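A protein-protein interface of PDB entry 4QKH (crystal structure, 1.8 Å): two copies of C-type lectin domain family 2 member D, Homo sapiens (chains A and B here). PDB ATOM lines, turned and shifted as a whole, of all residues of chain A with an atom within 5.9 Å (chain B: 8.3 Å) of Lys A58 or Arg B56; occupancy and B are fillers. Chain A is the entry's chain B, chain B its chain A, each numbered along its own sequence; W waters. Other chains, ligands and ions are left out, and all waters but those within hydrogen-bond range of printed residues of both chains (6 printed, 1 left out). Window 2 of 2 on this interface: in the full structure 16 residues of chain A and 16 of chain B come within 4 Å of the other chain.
The guanidinium group (NH1) of Arg A56 sits at hydrogen-bond distance from the backbone carbonyl oxygen (O) of Lys B58, at 3.0 Å. The guanidinium group (NH2) of Arg B56 is in hydrogen-bond range of the backbone carbonyl oxygen (O) of Lys A58 (3.1 Å). The guanidinium group of Arg B56 is in hydrogen-bond range of the backbone carbonyl oxygen of Tyr A57 (2.8 Å). NE of Arg A56 sits at hydrogen-bond distance from O of Tyr B57, 2.9 Å away.
The side-chain amino group of Lys B58 is in hydrogen-bond range of the backbone carbonyl oxygen of Asn B99 (2.8 Å). NZ of Lys A58 sits at hydrogen-bond distance from O of Ser A61 (2.9 Å).
Among the printed residues, pairs that only touch across the chains: Phe A21 with Arg B56, Phe A53 with Tyr B57, Arg A56 with Phe B21, Arg A56 with Arg B56, Tyr A57 with Phe B53 and Tyr A57 with Tyr B57.
Of the printed residues of chain B, Lys A58 touches Arg B56. Arg B56 touches just these residues of chain A: Phe A21 (3.8 Å), Arg A56 (3.8 Å), Tyr A57 (2.8 Å) and Lys A58 (3.1 Å). No residue of chain B comes within 4 Å of Gly A59. Printed residues of chain A within 4 Å of Lys B58: Arg A56. Printed residues of chain A within 4 Å of Tyr B57: Phe A53, Arg A56 and Tyr A57. Of the printed residues of chain A, Phe B21 touches Arg A56. Printed residues of chain B within 4 Å of Arg A56: Phe B21, Arg B56, Tyr B57 and Lys B58. Asp A100 touches none of the printed residues of chain B. The nearest residue of chain B that does not touch Lys A58 is Tyr B57 (6.6 Å). The nearest residue of chain A that does not touch Arg B56 is His A63 (4.3 Å).
Hydrophobic or aromatic side chains of chain A within 4 Å of the printed part of chain B: Phe A21, Phe A53 and Tyr A57. Of the 16 printed residues of chain B, 5 touch a printed residue of chain A. Hydrophobic or aromatic side chains of chain B within 4 Å of the printed part of chain A: Phe B21, Phe B53 and Tyr B57. Among the printed residues, no Asp or Glu carboxylate lies within 4 Å of a Lys or Arg side-chain nitrogen of the other chain.
Phe A53 touches Tyr B57, and with the chains exchanged Tyr A57 touches Phe B53. Arg A56 touches its own counterpart, Arg B56. Arg A56 touches Tyr B57, and with the chains exchanged Tyr A57 touches Arg B56. Arg A56 touches Lys B58, and with the chains exchanged Lys A58 touches Arg B56. Of the 10 pairs that touch across the chains among the printed residues, 10 have their exchanged pair printed and touching as well.
Water W4 lies within hydrogen-bond range of the backbone carbonyl oxygen (O) of Ser A22, a ring nitrogen (NE2) of His A63 and the guanidinium group (NH2) of Arg B56. Water W3 bridges O of Phe B21 (2.8 Å) and NH2 of Arg A56 (2.9 Å). Water W5 lies within hydrogen-bond range of O of Phe A21 (2.8 Å), NH1 of Arg B56 (2.9 Å) and OD1 of Asp A23 (3.0 Å). Water W6 lies within hydrogen-bond range of the backbone carbonyl oxygen of Arg B56 and the backbone carbonyl oxygen of Arg A56. Water W1 lies within hydrogen-bond range of the side-chain hydroxyl (OH) of Tyr A57 and the backbone NH (N) of Phe B53. Water W2 bridges the side-chain hydroxyl of Tyr B57 (3.1 Å) and the backbone NH of Phe A53 (3.5 Å).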
ATOM      1  N   PHE A  21      -6.417 -20.840  -0.579  1.00  0.00           N
ATOM      2  CA  PHE A  21      -7.171 -19.592  -0.495  1.00  0.00           C
ATOM      3  C   PHE A  21      -6.846 -18.824   0.780  1.00  0.00           C
ATOM      4  O   PHE A  21      -7.049 -19.318   1.893  1.00  0.00           O
ATOM      5  CB  PHE A  21      -8.682 -19.844  -0.554  1.00  0.00           C
ATOM      6  CG  PHE A  21      -9.161 -20.413  -1.871  1.00  0.00           C
ATOM      7  CD1 PHE A  21      -8.877 -21.743  -2.175  1.00  0.00           C
ATOM      8  CD2 PHE A  21      -9.877 -19.654  -2.771  1.00  0.00           C
ATOM      9  CE1 PHE A  21      -9.302 -22.314  -3.369  1.00  0.00           C
ATOM     10  CE2 PHE A  21     -10.333 -20.263  -3.973  1.00  0.00           C
ATOM     11  CZ  PHE A  21     -10.003 -21.569  -4.255  1.00  0.00           C
ATOM     12  N   SER A  22      -6.394 -17.595   0.642  1.00  0.00           N
ATOM     13  CA  SER A  22      -5.882 -16.869   1.794  1.00  0.00           C
ATOM     14  C   SER A  22      -6.954 -16.349   2.754  1.00  0.00           C
ATOM     15  O   SER A  22      -8.121 -16.158   2.396  1.00  0.00           O
ATOM     16  CB  SER A  22      -4.989 -15.723   1.323  1.00  0.00           C
ATOM     17  OG  SER A  22      -5.781 -14.590   0.945  1.00  0.00           O
ATOM     18  N   ASP A  23      -6.529 -16.102   3.985  1.00  0.00           N
ATOM     19  CA  ASP A  23      -7.375 -15.440   4.973  1.00  0.00           C
ATOM     20  C   ASP A  23      -7.053 -13.951   5.042  1.00  0.00           C
ATOM     21  O   ASP A  23      -7.911 -13.120   5.325  1.00  0.00           O
ATOM     22  CB  ASP A  23      -7.196 -16.085   6.322  1.00  0.00           C
ATOM     23  CG  ASP A  23      -7.801 -17.463   6.385  1.00  0.00           C
ATOM     24  OD1 ASP A  23      -8.893 -17.663   5.791  1.00  0.00           O
ATOM     25  OD2 ASP A  23      -7.181 -18.336   7.041  1.00  0.00           O
ATOM     26  N   PHE A  53     -14.556 -23.704 -10.681  1.00  0.00           N
ATOM     27  CA  PHE A  53     -14.220 -24.290  -9.406  1.00  0.00           C
ATOM     28  C   PHE A  53     -13.773 -23.171  -8.407  1.00  0.00           C
ATOM     29  O   PHE A  53     -14.240 -23.058  -7.286  1.00  0.00           O
ATOM     30  CB  PHE A  53     -13.106 -25.346  -9.576  1.00  0.00           C
ATOM     31  CG  PHE A  53     -12.330 -25.588  -8.309  1.00  0.00           C
ATOM     32  CD1 PHE A  53     -12.955 -26.218  -7.241  1.00  0.00           C
ATOM     33  CD2 PHE A  53     -11.028 -25.147  -8.152  1.00  0.00           C
ATOM     34  CE1 PHE A  53     -12.275 -26.396  -6.040  1.00  0.00           C
ATOM     35  CE2 PHE A  53     -10.327 -25.347  -6.956  1.00  0.00           C
ATOM     36  CZ  PHE A  53     -10.952 -25.965  -5.909  1.00  0.00           C
ATOM     37  N   LEU A  54     -12.823 -22.342  -8.816  1.00  0.00           N
ATOM     38  CA  LEU A  54     -12.327 -21.281  -7.960  1.00  0.00           C
ATOM     39  C   LEU A  54     -13.484 -20.314  -7.574  1.00  0.00           C
ATOM     40  O   LEU A  54     -13.543 -19.893  -6.438  1.00  0.00           O
ATOM     41  CB  LEU A  54     -11.220 -20.500  -8.648  1.00  0.00           C
ATOM     42  CG  LEU A  54      -9.979 -21.337  -8.950  1.00  0.00           C
ATOM     43  CD1 LEU A  54      -9.041 -20.458  -9.762  1.00  0.00           C
ATOM     44  CD2 LEU A  54      -9.370 -21.787  -7.646  1.00  0.00           C
ATOM     45  N   LEU A  55     -14.304 -19.930  -8.541  1.00  0.00           N
ATOM     46  CA  LEU A  55     -15.423 -18.986  -8.281  1.00  0.00           C
ATOM     47  C   LEU A  55     -16.433 -19.559  -7.334  1.00  0.00           C
ATOM     48  O   LEU A  55     -16.997 -18.795  -6.535  1.00  0.00           O
ATOM     49  CB  LEU A  55     -16.078 -18.515  -9.585  1.00  0.00           C
ATOM     50  CG  LEU A  55     -15.230 -17.671 -10.499  1.00  0.00           C
ATOM     51  CD1 LEU A  55     -15.880 -17.418 -11.861  1.00  0.00           C
ATOM     52  CD2 LEU A  55     -14.979 -16.390  -9.745  1.00  0.00           C
ATOM     53  N   ARG A  56     -16.684 -20.888  -7.366  1.00  0.00           N
ATOM     54  CA  ARG A  56     -17.608 -21.501  -6.414  1.00  0.00           C
ATOM     55  C   ARG A  56     -17.077 -21.433  -4.953  1.00  0.00           C
ATOM     56  O   ARG A  56     -17.819 -21.158  -4.020  1.00  0.00           O
ATOM     57  CB  ARG A  56     -17.904 -22.930  -6.811  1.00  0.00           C
ATOM     58  CG  ARG A  56     -18.933 -23.678  -5.947  1.00  0.00           C
ATOM     59  CD  ARG A  56     -19.414 -24.921  -6.599  1.00  0.00           C
ATOM     60  NE  ARG A  56     -20.392 -25.598  -5.759  1.00  0.00           N
ATOM     61  CZ  ARG A  56     -21.054 -26.686  -6.054  1.00  0.00           C
ATOM     62  NH1 ARG A  56     -21.817 -27.200  -5.113  1.00  0.00           N
ATOM     63  NH2 ARG A  56     -20.914 -27.290  -7.228  1.00  0.00           N
ATOM     64  N   TYR A  57     -15.800 -21.717  -4.750  1.00  0.00           N
ATOM     65  CA  TYR A  57     -15.210 -21.734  -3.451  1.00  0.00           C
ATOM     66  C   TYR A  57     -14.857 -20.413  -2.861  1.00  0.00           C
ATOM     67  O   TYR A  57     -14.756 -20.304  -1.605  1.00  0.00           O
ATOM     68  CB  TYR A  57     -13.943 -22.651  -3.428  1.00  0.00           C
ATOM     69  CG  TYR A  57     -13.455 -22.947  -2.016  1.00  0.00           C
ATOM     70  CD1 TYR A  57     -14.157 -23.814  -1.182  1.00  0.00           C
ATOM     71  CD2 TYR A  57     -12.341 -22.285  -1.481  1.00  0.00           C
ATOM     72  CE1 TYR A  57     -13.750 -24.063   0.123  1.00  0.00           C
ATOM     73  CE2 TYR A  57     -11.904 -22.539  -0.181  1.00  0.00           C
ATOM     74  CZ  TYR A  57     -12.603 -23.444   0.617  1.00  0.00           C
ATOM     75  OH  TYR A  57     -12.186 -23.683   1.887  1.00  0.00           O
ATOM     76  N   LYS A  58     -14.562 -19.435  -3.683  1.00  0.00           N
ATOM     77  CA  LYS A  58     -13.770 -18.324  -3.141  1.00  0.00           C
ATOM     78  C   LYS A  58     -14.543 -17.433  -2.170  1.00  0.00           C
ATOM     79  O   LYS A  58     -13.923 -16.866  -1.286  1.00  0.00           O
ATOM     80  CB  LYS A  58     -13.151 -17.420  -4.196  1.00  0.00           C
ATOM     81  CG  LYS A  58     -14.065 -16.632  -5.023  1.00  0.00           C
ATOM     82  CD  LYS A  58     -13.362 -15.435  -5.734  1.00  0.00           C
ATOM     83  CE  LYS A  58     -14.399 -14.511  -6.323  1.00  0.00           C
ATOM     84  NZ  LYS A  58     -14.850 -13.460  -5.369  1.00  0.00           N
ATOM     85  N   GLY A  59     -15.840 -17.325  -2.360  1.00  0.00           N
ATOM     86  CA  GLY A  59     -16.669 -16.396  -1.550  1.00  0.00           C
ATOM     87  C   GLY A  59     -16.540 -14.978  -2.050  1.00  0.00           C
ATOM     88  O   GLY A  59     -15.987 -14.736  -3.125  1.00  0.00           O
ATOM     89  N   PRO A  60     -17.105 -13.997  -1.306  1.00  0.00           N
ATOM     90  CA  PRO A  60     -17.307 -12.660  -1.887  1.00  0.00           C
ATOM     91  C   PRO A  60     -16.070 -11.749  -2.041  1.00  0.00           C
ATOM     92  O   PRO A  60     -16.133 -10.843  -2.852  1.00  0.00           O
ATOM     93  CB  PRO A  60     -18.366 -12.025  -0.938  1.00  0.00           C
ATOM     94  CG  PRO A  60     -18.160 -12.729   0.324  1.00  0.00           C
ATOM     95  CD  PRO A  60     -17.842 -14.140  -0.053  1.00  0.00           C
ATOM     96  N   SER A  61     -14.973 -12.016  -1.332  1.00  0.00           N
ATOM     97  CA  SER A  61     -13.737 -11.242  -1.470  1.00  0.00           C
ATOM     98  C   SER A  61     -13.014 -11.342  -2.809  1.00  0.00           C
ATOM     99  O   SER A  61     -12.971 -12.442  -3.425  1.00  0.00           O
ATOM    100  CB  SER A  61     -12.766 -11.616  -0.353  1.00  0.00           C
ATOM    101  OG  SER A  61     -13.354 -11.358   0.877  1.00  0.00           O
ATOM    102  N   ASP A  62     -12.444 -10.223  -3.281  1.00  0.00           N
ATOM    103  CA  ASP A  62     -11.596 -10.250  -4.453  1.00  0.00           C
ATOM    104  C   ASP A  62     -10.350 -11.107  -4.126  1.00  0.00           C
ATOM    105  O   ASP A  62      -9.825 -11.040  -2.996  1.00  0.00           O
ATOM    106  CB  ASP A  62     -11.137  -8.874  -4.882  1.00  0.00           C
ATOM    107  CG  ASP A  62     -12.286  -7.969  -5.338  1.00  0.00           C
ATOM    108  OD1 ASP A  62     -13.388  -8.495  -5.624  1.00  0.00           O
ATOM    109  OD2 ASP A  62     -12.014  -6.754  -5.410  1.00  0.00           O
ATOM    110  N   HIS A  63      -9.899 -11.886  -5.098  1.00  0.00           N
ATOM    111  CA  HIS A  63      -8.717 -12.781  -4.919  1.00  0.00           C
ATOM    112  C   HIS A  63      -7.720 -12.632  -6.079  1.00  0.00           C
ATOM    113  O   HIS A  63      -8.038 -12.957  -7.255  1.00  0.00           O
ATOM    114  CB  HIS A  63      -9.168 -14.233  -4.819  1.00  0.00           C
ATOM    115  CG  HIS A  63      -9.703 -14.646  -3.485  1.00  0.00           C
ATOM    116  ND1 HIS A  63     -10.968 -14.291  -3.018  1.00  0.00           N
ATOM    117  CD2 HIS A  63      -9.151 -15.391  -2.515  1.00  0.00           C
ATOM    118  CE1 HIS A  63     -11.159 -14.841  -1.847  1.00  0.00           C
ATOM    119  NE2 HIS A  63     -10.083 -15.524  -1.525  1.00  0.00           N
ATOM    120  N   LEU A  98      -9.853 -12.415  -9.279  1.00  0.00           N
ATOM    121  CA  LEU A  98     -11.171 -12.967  -9.419  1.00  0.00           C
ATOM    122  C   LEU A  98     -12.145 -12.202  -8.581  1.00  0.00           C
ATOM    123  O   LEU A  98     -11.944 -11.990  -7.396  1.00  0.00           O
ATOM    124  CB  LEU A  98     -11.279 -14.437  -9.070  1.00  0.00           C
ATOM    125  CG  LEU A  98     -10.492 -15.374  -9.962  1.00  0.00           C
ATOM    126  CD1 LEU A  98     -10.696 -16.818  -9.579  1.00  0.00           C
ATOM    127  CD2 LEU A  98     -10.804 -15.151 -11.423  1.00  0.00           C
ATOM    128  N   ASN A  99     -13.165 -11.682  -9.245  1.00  0.00           N
ATOM    129  CA  ASN A  99     -14.330 -11.182  -8.512  1.00  0.00           C
ATOM    130  C   ASN A  99     -15.497 -12.194  -8.705  1.00  0.00           C
ATOM    131  O   ASN A  99     -15.311 -13.268  -9.283  1.00  0.00           O
ATOM    132  CB  ASN A  99     -14.675  -9.731  -8.877  1.00  0.00           C
ATOM    133  CG  ASN A  99     -15.106  -9.574 -10.329  1.00  0.00           C
ATOM    134  OD1 ASN A  99     -15.603 -10.524 -10.959  1.00  0.00           O
ATOM    135  ND2 ASN A  99     -14.910  -8.392 -10.865  1.00  0.00           N
ATOM    136  N   ASP A 100     -16.693 -11.834  -8.274  1.00  0.00           N
ATOM    137  CA  ASP A 100     -17.830 -12.770  -8.276  1.00  0.00           C
ATOM    138  C   ASP A 100     -18.325 -13.169  -9.680  1.00  0.00           C
ATOM    139  O   ASP A 100     -18.991 -14.195  -9.829  1.00  0.00           O
ATOM    140  CB  ASP A 100     -19.005 -12.193  -7.482  1.00  0.00           C
ATOM    141  CG  ASP A 100     -19.585 -10.976  -8.145  1.00  0.00           C
ATOM    142  OD1 ASP A 100     -18.791 -10.200  -8.702  1.00  0.00           O
ATOM    143  OD2 ASP A 100     -20.817 -10.791  -8.125  1.00  0.00           O
ATOM    144  N   ILE A 115      -5.111 -16.437  -4.199  1.00  0.00           N
ATOM    145  CA  ILE A 115      -5.060 -17.892  -4.418  1.00  0.00           C
ATOM    146  C   ILE A 115      -3.683 -18.339  -4.924  1.00  0.00           C
ATOM    147  O   ILE A 115      -3.213 -17.806  -5.938  1.00  0.00           O
ATOM    148  CB  ILE A 115      -6.167 -18.258  -5.417  1.00  0.00           C
ATOM    149  CG1 ILE A 115      -7.509 -17.604  -5.002  1.00  0.00           C
ATOM    150  CG2 ILE A 115      -6.266 -19.761  -5.620  1.00  0.00           C
ATOM    151  CD1 ILE A 115      -8.621 -17.813  -6.012  1.00  0.00           C
ATOM    152  N   PHE B  21     -20.506 -33.107  -4.728  1.00  0.00           N
ATOM    153  CA  PHE B  21     -21.619 -32.208  -4.404  1.00  0.00           C
ATOM    154  C   PHE B  21     -22.659 -32.401  -5.505  1.00  0.00           C
ATOM    155  O   PHE B  21     -22.468 -32.073  -6.698  1.00  0.00           O
ATOM    156  CB  PHE B  21     -21.142 -30.774  -4.262  1.00  0.00           C
ATOM    157  CG  PHE B  21     -20.096 -30.583  -3.207  1.00  0.00           C
ATOM    158  CD1 PHE B  21     -18.759 -30.920  -3.432  1.00  0.00           C
ATOM    159  CD2 PHE B  21     -20.435 -30.044  -1.979  1.00  0.00           C
ATOM    160  CE1 PHE B  21     -17.818 -30.725  -2.479  1.00  0.00           C
ATOM    161  CE2 PHE B  21     -19.478 -29.849  -1.013  1.00  0.00           C
ATOM    162  CZ  PHE B  21     -18.153 -30.208  -1.259  1.00  0.00           C
ATOM    163  N   GLN B  49     -12.918 -28.032  10.598  1.00  0.00           N
ATOM    164  CA  GLN B  49     -12.347 -27.484   9.376  1.00  0.00           C
ATOM    165  C   GLN B  49     -13.047 -28.134   8.164  1.00  0.00           C
ATOM    166  O   GLN B  49     -13.152 -27.538   7.123  1.00  0.00           O
ATOM    167  CB  GLN B  49     -10.816 -27.703   9.281  1.00  0.00           C
ATOM    168  CG  GLN B  49     -10.016 -27.266  10.507  1.00  0.00           C
ATOM    169  CD  GLN B  49      -9.729 -28.447  11.447  1.00  0.00           C
ATOM    170  OE1 GLN B  49      -8.801 -29.229  11.215  1.00  0.00           O
ATOM    171  NE2 GLN B  49     -10.535 -28.591  12.490  1.00  0.00           N
ATOM    172  N   GLU B  50     -13.477 -29.376   8.305  1.00  0.00           N
ATOM    173  CA  GLU B  50     -14.141 -30.058   7.186  1.00  0.00           C
ATOM    174  C   GLU B  50     -15.549 -29.479   7.032  1.00  0.00           C
ATOM    175  O   GLU B  50     -16.006 -29.208   5.919  1.00  0.00           O
ATOM    176  CB  GLU B  50     -14.151 -31.572   7.419  1.00  0.00           C
ATOM    177  CG  GLU B  50     -14.560 -32.388   6.212  1.00  0.00           C
ATOM    178  CD  GLU B  50     -14.867 -33.840   6.577  1.00  0.00           C
ATOM    179  OE1 GLU B  50     -15.748 -34.424   5.913  1.00  0.00           O
ATOM    180  OE2 GLU B  50     -14.256 -34.376   7.551  1.00  0.00           O
ATOM    181  N   LEU B  51     -16.217 -29.254   8.147  1.00  0.00           N
ATOM    182  CA  LEU B  51     -17.510 -28.591   8.168  1.00  0.00           C
ATOM    183  C   LEU B  51     -17.475 -27.235   7.454  1.00  0.00           C
ATOM    184  O   LEU B  51     -18.325 -26.950   6.606  1.00  0.00           O
ATOM    185  CB  LEU B  51     -18.030 -28.388   9.604  1.00  0.00           C
ATOM    186  CG  LEU B  51     -19.237 -27.425   9.755  1.00  0.00           C
ATOM    187  CD1 LEU B  51     -20.485 -27.934   9.039  1.00  0.00           C
ATOM    188  CD2 LEU B  51     -19.631 -27.180  11.208  1.00  0.00           C
ATOM    189  N   ASN B  52     -16.516 -26.392   7.849  1.00  0.00           N
ATOM    190  CA  ASN B  52     -16.320 -25.105   7.207  1.00  0.00           C
ATOM    191  C   ASN B  52     -16.039 -25.215   5.701  1.00  0.00           C
ATOM    192  O   ASN B  52     -16.612 -24.452   4.931  1.00  0.00           O
ATOM    193  CB  ASN B  52     -15.186 -24.324   7.923  1.00  0.00           C
ATOM    194  CG  ASN B  52     -15.603 -23.816   9.292  1.00  0.00           C
ATOM    195  OD1 ASN B  52     -16.790 -23.702   9.582  1.00  0.00           O
ATOM    196  ND2 ASN B  52     -14.630 -23.517  10.140  1.00  0.00           N
ATOM    197  N   PHE B  53     -15.206 -26.178   5.292  1.00  0.00           N
ATOM    198  CA  PHE B  53     -14.918 -26.425   3.889  1.00  0.00           C
ATOM    199  C   PHE B  53     -16.220 -26.739   3.129  1.00  0.00           C
ATOM    200  O   PHE B  53     -16.483 -26.195   2.064  1.00  0.00           O
ATOM    201  CB  PHE B  53     -13.833 -27.546   3.689  1.00  0.00           C
ATOM    202  CG  PHE B  53     -13.825 -28.136   2.281  1.00  0.00           C
ATOM    203  CD1 PHE B  53     -13.292 -27.400   1.192  1.00  0.00           C
ATOM    204  CD2 PHE B  53     -14.411 -29.380   2.021  1.00  0.00           C
ATOM    205  CE1 PHE B  53     -13.359 -27.934  -0.123  1.00  0.00           C
ATOM    206  CE2 PHE B  53     -14.437 -29.893   0.756  1.00  0.00           C
ATOM    207  CZ  PHE B  53     -13.939 -29.178  -0.316  1.00  0.00           C
ATOM    208  N   LEU B  54     -17.055 -27.634   3.686  1.00  0.00           N
ATOM    209  CA  LEU B  54     -18.305 -28.030   2.985  1.00  0.00           C
ATOM    210  C   LEU B  54     -19.305 -26.872   2.939  1.00  0.00           C
ATOM    211  O   LEU B  54     -19.945 -26.589   1.908  1.00  0.00           O
ATOM    212  CB  LEU B  54     -18.958 -29.252   3.669  1.00  0.00           C
ATOM    213  CG  LEU B  54     -18.042 -30.495   3.669  1.00  0.00           C
ATOM    214  CD1 LEU B  54     -18.619 -31.621   4.543  1.00  0.00           C
ATOM    215  CD2 LEU B  54     -17.698 -30.985   2.267  1.00  0.00           C
ATOM    216  N   LEU B  55     -19.426 -26.147   4.018  1.00  0.00           N
ATOM    217  CA  LEU B  55     -20.318 -24.984   4.022  1.00  0.00           C
ATOM    218  C   LEU B  55     -19.911 -23.975   2.953  1.00  0.00           C
ATOM    219  O   LEU B  55     -20.769 -23.332   2.314  1.00  0.00           O
ATOM    220  CB  LEU B  55     -20.347 -24.367   5.401  1.00  0.00           C
ATOM    221  CG  LEU B  55     -20.995 -25.162   6.536  1.00  0.00           C
ATOM    222  CD1 LEU B  55     -20.828 -24.400   7.859  1.00  0.00           C
ATOM    223  CD2 LEU B  55     -22.460 -25.333   6.271  1.00  0.00           C
ATOM    224  N   ARG B  56     -18.610 -23.839   2.754  1.00  0.00           N
ATOM    225  CA  ARG B  56     -18.071 -22.834   1.841  1.00  0.00           C
ATOM    226  C   ARG B  56     -18.223 -23.224   0.414  1.00  0.00           C
ATOM    227  O   ARG B  56     -18.474 -22.379  -0.443  1.00  0.00           O
ATOM    228  CB  ARG B  56     -16.613 -22.556   2.182  1.00  0.00           C
ATOM    229  CG  ARG B  56     -15.971 -21.458   1.339  1.00  0.00           C
ATOM    230  CD  ARG B  56     -14.649 -20.995   1.993  1.00  0.00           C
ATOM    231  NE  ARG B  56     -13.945 -20.083   1.092  1.00  0.00           N
ATOM    232  CZ  ARG B  56     -12.760 -19.550   1.346  1.00  0.00           C
ATOM    233  NH1 ARG B  56     -12.124 -19.851   2.475  1.00  0.00           N
ATOM    234  NH2 ARG B  56     -12.198 -18.753   0.462  1.00  0.00           N
ATOM    235  N   TYR B  57     -18.013 -24.493   0.078  1.00  0.00           N
ATOM    236  CA  TYR B  57     -18.100 -24.924  -1.314  1.00  0.00           C
ATOM    237  C   TYR B  57     -19.546 -25.206  -1.802  1.00  0.00           C
ATOM    238  O   TYR B  57     -19.882 -24.963  -2.979  1.00  0.00           O
ATOM    239  CB  TYR B  57     -17.255 -26.205  -1.541  1.00  0.00           C
ATOM    240  CG  TYR B  57     -17.152 -26.541  -3.022  1.00  0.00           C
ATOM    241  CD1 TYR B  57     -16.225 -25.871  -3.817  1.00  0.00           C
ATOM    242  CD2 TYR B  57     -17.983 -27.459  -3.644  1.00  0.00           C
ATOM    243  CE1 TYR B  57     -16.113 -26.136  -5.192  1.00  0.00           C
ATOM    244  CE2 TYR B  57     -17.858 -27.750  -5.020  1.00  0.00           C
ATOM    245  CZ  TYR B  57     -16.895 -27.058  -5.781  1.00  0.00           C
ATOM    246  OH  TYR B  57     -16.718 -27.239  -7.145  1.00  0.00           O
ATOM    247  N   LYS B  58     -20.434 -25.639  -0.883  1.00  0.00           N
ATOM    248  CA  LYS B  58     -21.696 -26.270  -1.318  1.00  0.00           C
ATOM    249  C   LYS B  58     -22.728 -25.397  -2.074  1.00  0.00           C
ATOM    250  O   LYS B  58     -23.440 -25.870  -2.993  1.00  0.00           O
ATOM    251  CB  LYS B  58     -22.363 -26.959  -0.145  1.00  0.00           C
ATOM    252  CG  LYS B  58     -23.118 -26.086   0.803  1.00  0.00           C
ATOM    253  CD  LYS B  58     -23.668 -26.869   1.985  1.00  0.00           C
ATOM    254  CE  LYS B  58     -24.508 -25.983   2.890  1.00  0.00           C
ATOM    255  NZ  LYS B  58     -25.486 -25.101   2.239  1.00  0.00           N
ATOM    256  N   GLY B  59     -22.784 -24.131  -1.705  1.00  0.00           N
ATOM    257  CA  GLY B  59     -23.677 -23.162  -2.305  1.00  0.00           C
ATOM    258  C   GLY B  59     -24.911 -22.985  -1.386  1.00  0.00           C
ATOM    259  O   GLY B  59     -24.919 -23.470  -0.284  1.00  0.00           O
ATOM    260  N   PRO B  60     -25.958 -22.320  -1.874  1.00  0.00           N
ATOM    261  CA  PRO B  60     -27.143 -21.935  -1.077  1.00  0.00           C
ATOM    262  C   PRO B  60     -28.079 -23.073  -0.625  1.00  0.00           C
ATOM    263  O   PRO B  60     -28.790 -22.882   0.410  1.00  0.00           O
ATOM    264  CB  PRO B  60     -27.884 -20.963  -1.994  1.00  0.00           C
ATOM    265  CG  PRO B  60     -27.491 -21.351  -3.374  1.00  0.00           C
ATOM    266  CD  PRO B  60     -26.127 -21.994  -3.295  1.00  0.00           C
ATOM    267  N   LEU B  98     -26.625 -29.898   6.112  1.00  0.00           N
ATOM    268  CA  LEU B  98     -26.002 -28.609   6.241  1.00  0.00           C
ATOM    269  C   LEU B  98     -26.903 -27.611   5.567  1.00  0.00           C
ATOM    270  O   LEU B  98     -27.332 -27.800   4.398  1.00  0.00           O
ATOM    271  CB  LEU B  98     -24.621 -28.623   5.589  1.00  0.00           C
ATOM    272  CG  LEU B  98     -23.596 -29.664   5.970  1.00  0.00           C
ATOM    273  CD1 LEU B  98     -22.331 -29.436   5.186  1.00  0.00           C
ATOM    274  CD2 LEU B  98     -23.306 -29.725   7.474  1.00  0.00           C
ATOM    275  N   ASN B  99     -27.260 -26.566   6.318  1.00  0.00           N
ATOM    276  CA  ASN B  99     -27.999 -25.451   5.747  1.00  0.00           C
ATOM    277  C   ASN B  99     -27.079 -24.309   5.296  1.00  0.00           C
ATOM    278  O   ASN B  99     -25.938 -24.534   4.960  1.00  0.00           O
ATOM    279  CB  ASN B  99     -29.175 -25.000   6.654  1.00  0.00           C
ATOM    280  CG  ASN B  99     -28.748 -24.370   7.986  1.00  0.00           C
ATOM    281  OD1 ASN B  99     -27.590 -24.098   8.273  1.00  0.00           O
ATOM    282  ND2 ASN B  99     -29.754 -24.111   8.806  1.00  0.00           N
ATOM    283  N   ASP B 100     -27.583 -23.076   5.289  1.00  0.00           N
ATOM    284  CA  ASP B 100     -26.824 -21.941   4.820  1.00  0.00           C
ATOM    285  C   ASP B 100     -25.793 -21.521   5.845  1.00  0.00           C
ATOM    286  O   ASP B 100     -24.790 -20.959   5.459  1.00  0.00           O
ATOM    287  CB  ASP B 100     -27.746 -20.759   4.392  1.00  0.00           C
ATOM    288  CG  ASP B 100     -28.743 -20.349   5.468  1.00  0.00           C
ATOM    289  OD1 ASP B 100     -29.521 -21.243   5.917  1.00  0.00           O
ATOM    290  OD2 ASP B 100     -28.752 -19.120   5.837  1.00  0.00           O
HETATM  291  O   HOH W   1     -13.015 -23.740   4.714  1.00  0.00           O
HETATM  292  O   HOH W   2     -17.095 -25.966  -9.917  1.00  0.00           O
HETATM  293  O   HOH W   3     -22.647 -29.579  -7.868  1.00  0.00           O
HETATM  294  O   HOH W   4     -10.034 -16.864   0.989  1.00  0.00           O
HETATM  295  O   HOH W   5      -9.436 -19.429   3.434  1.00  0.00           O
HETATM  296  O   HOH W   6     -18.242 -19.622  -1.151  1.00  0.00           O
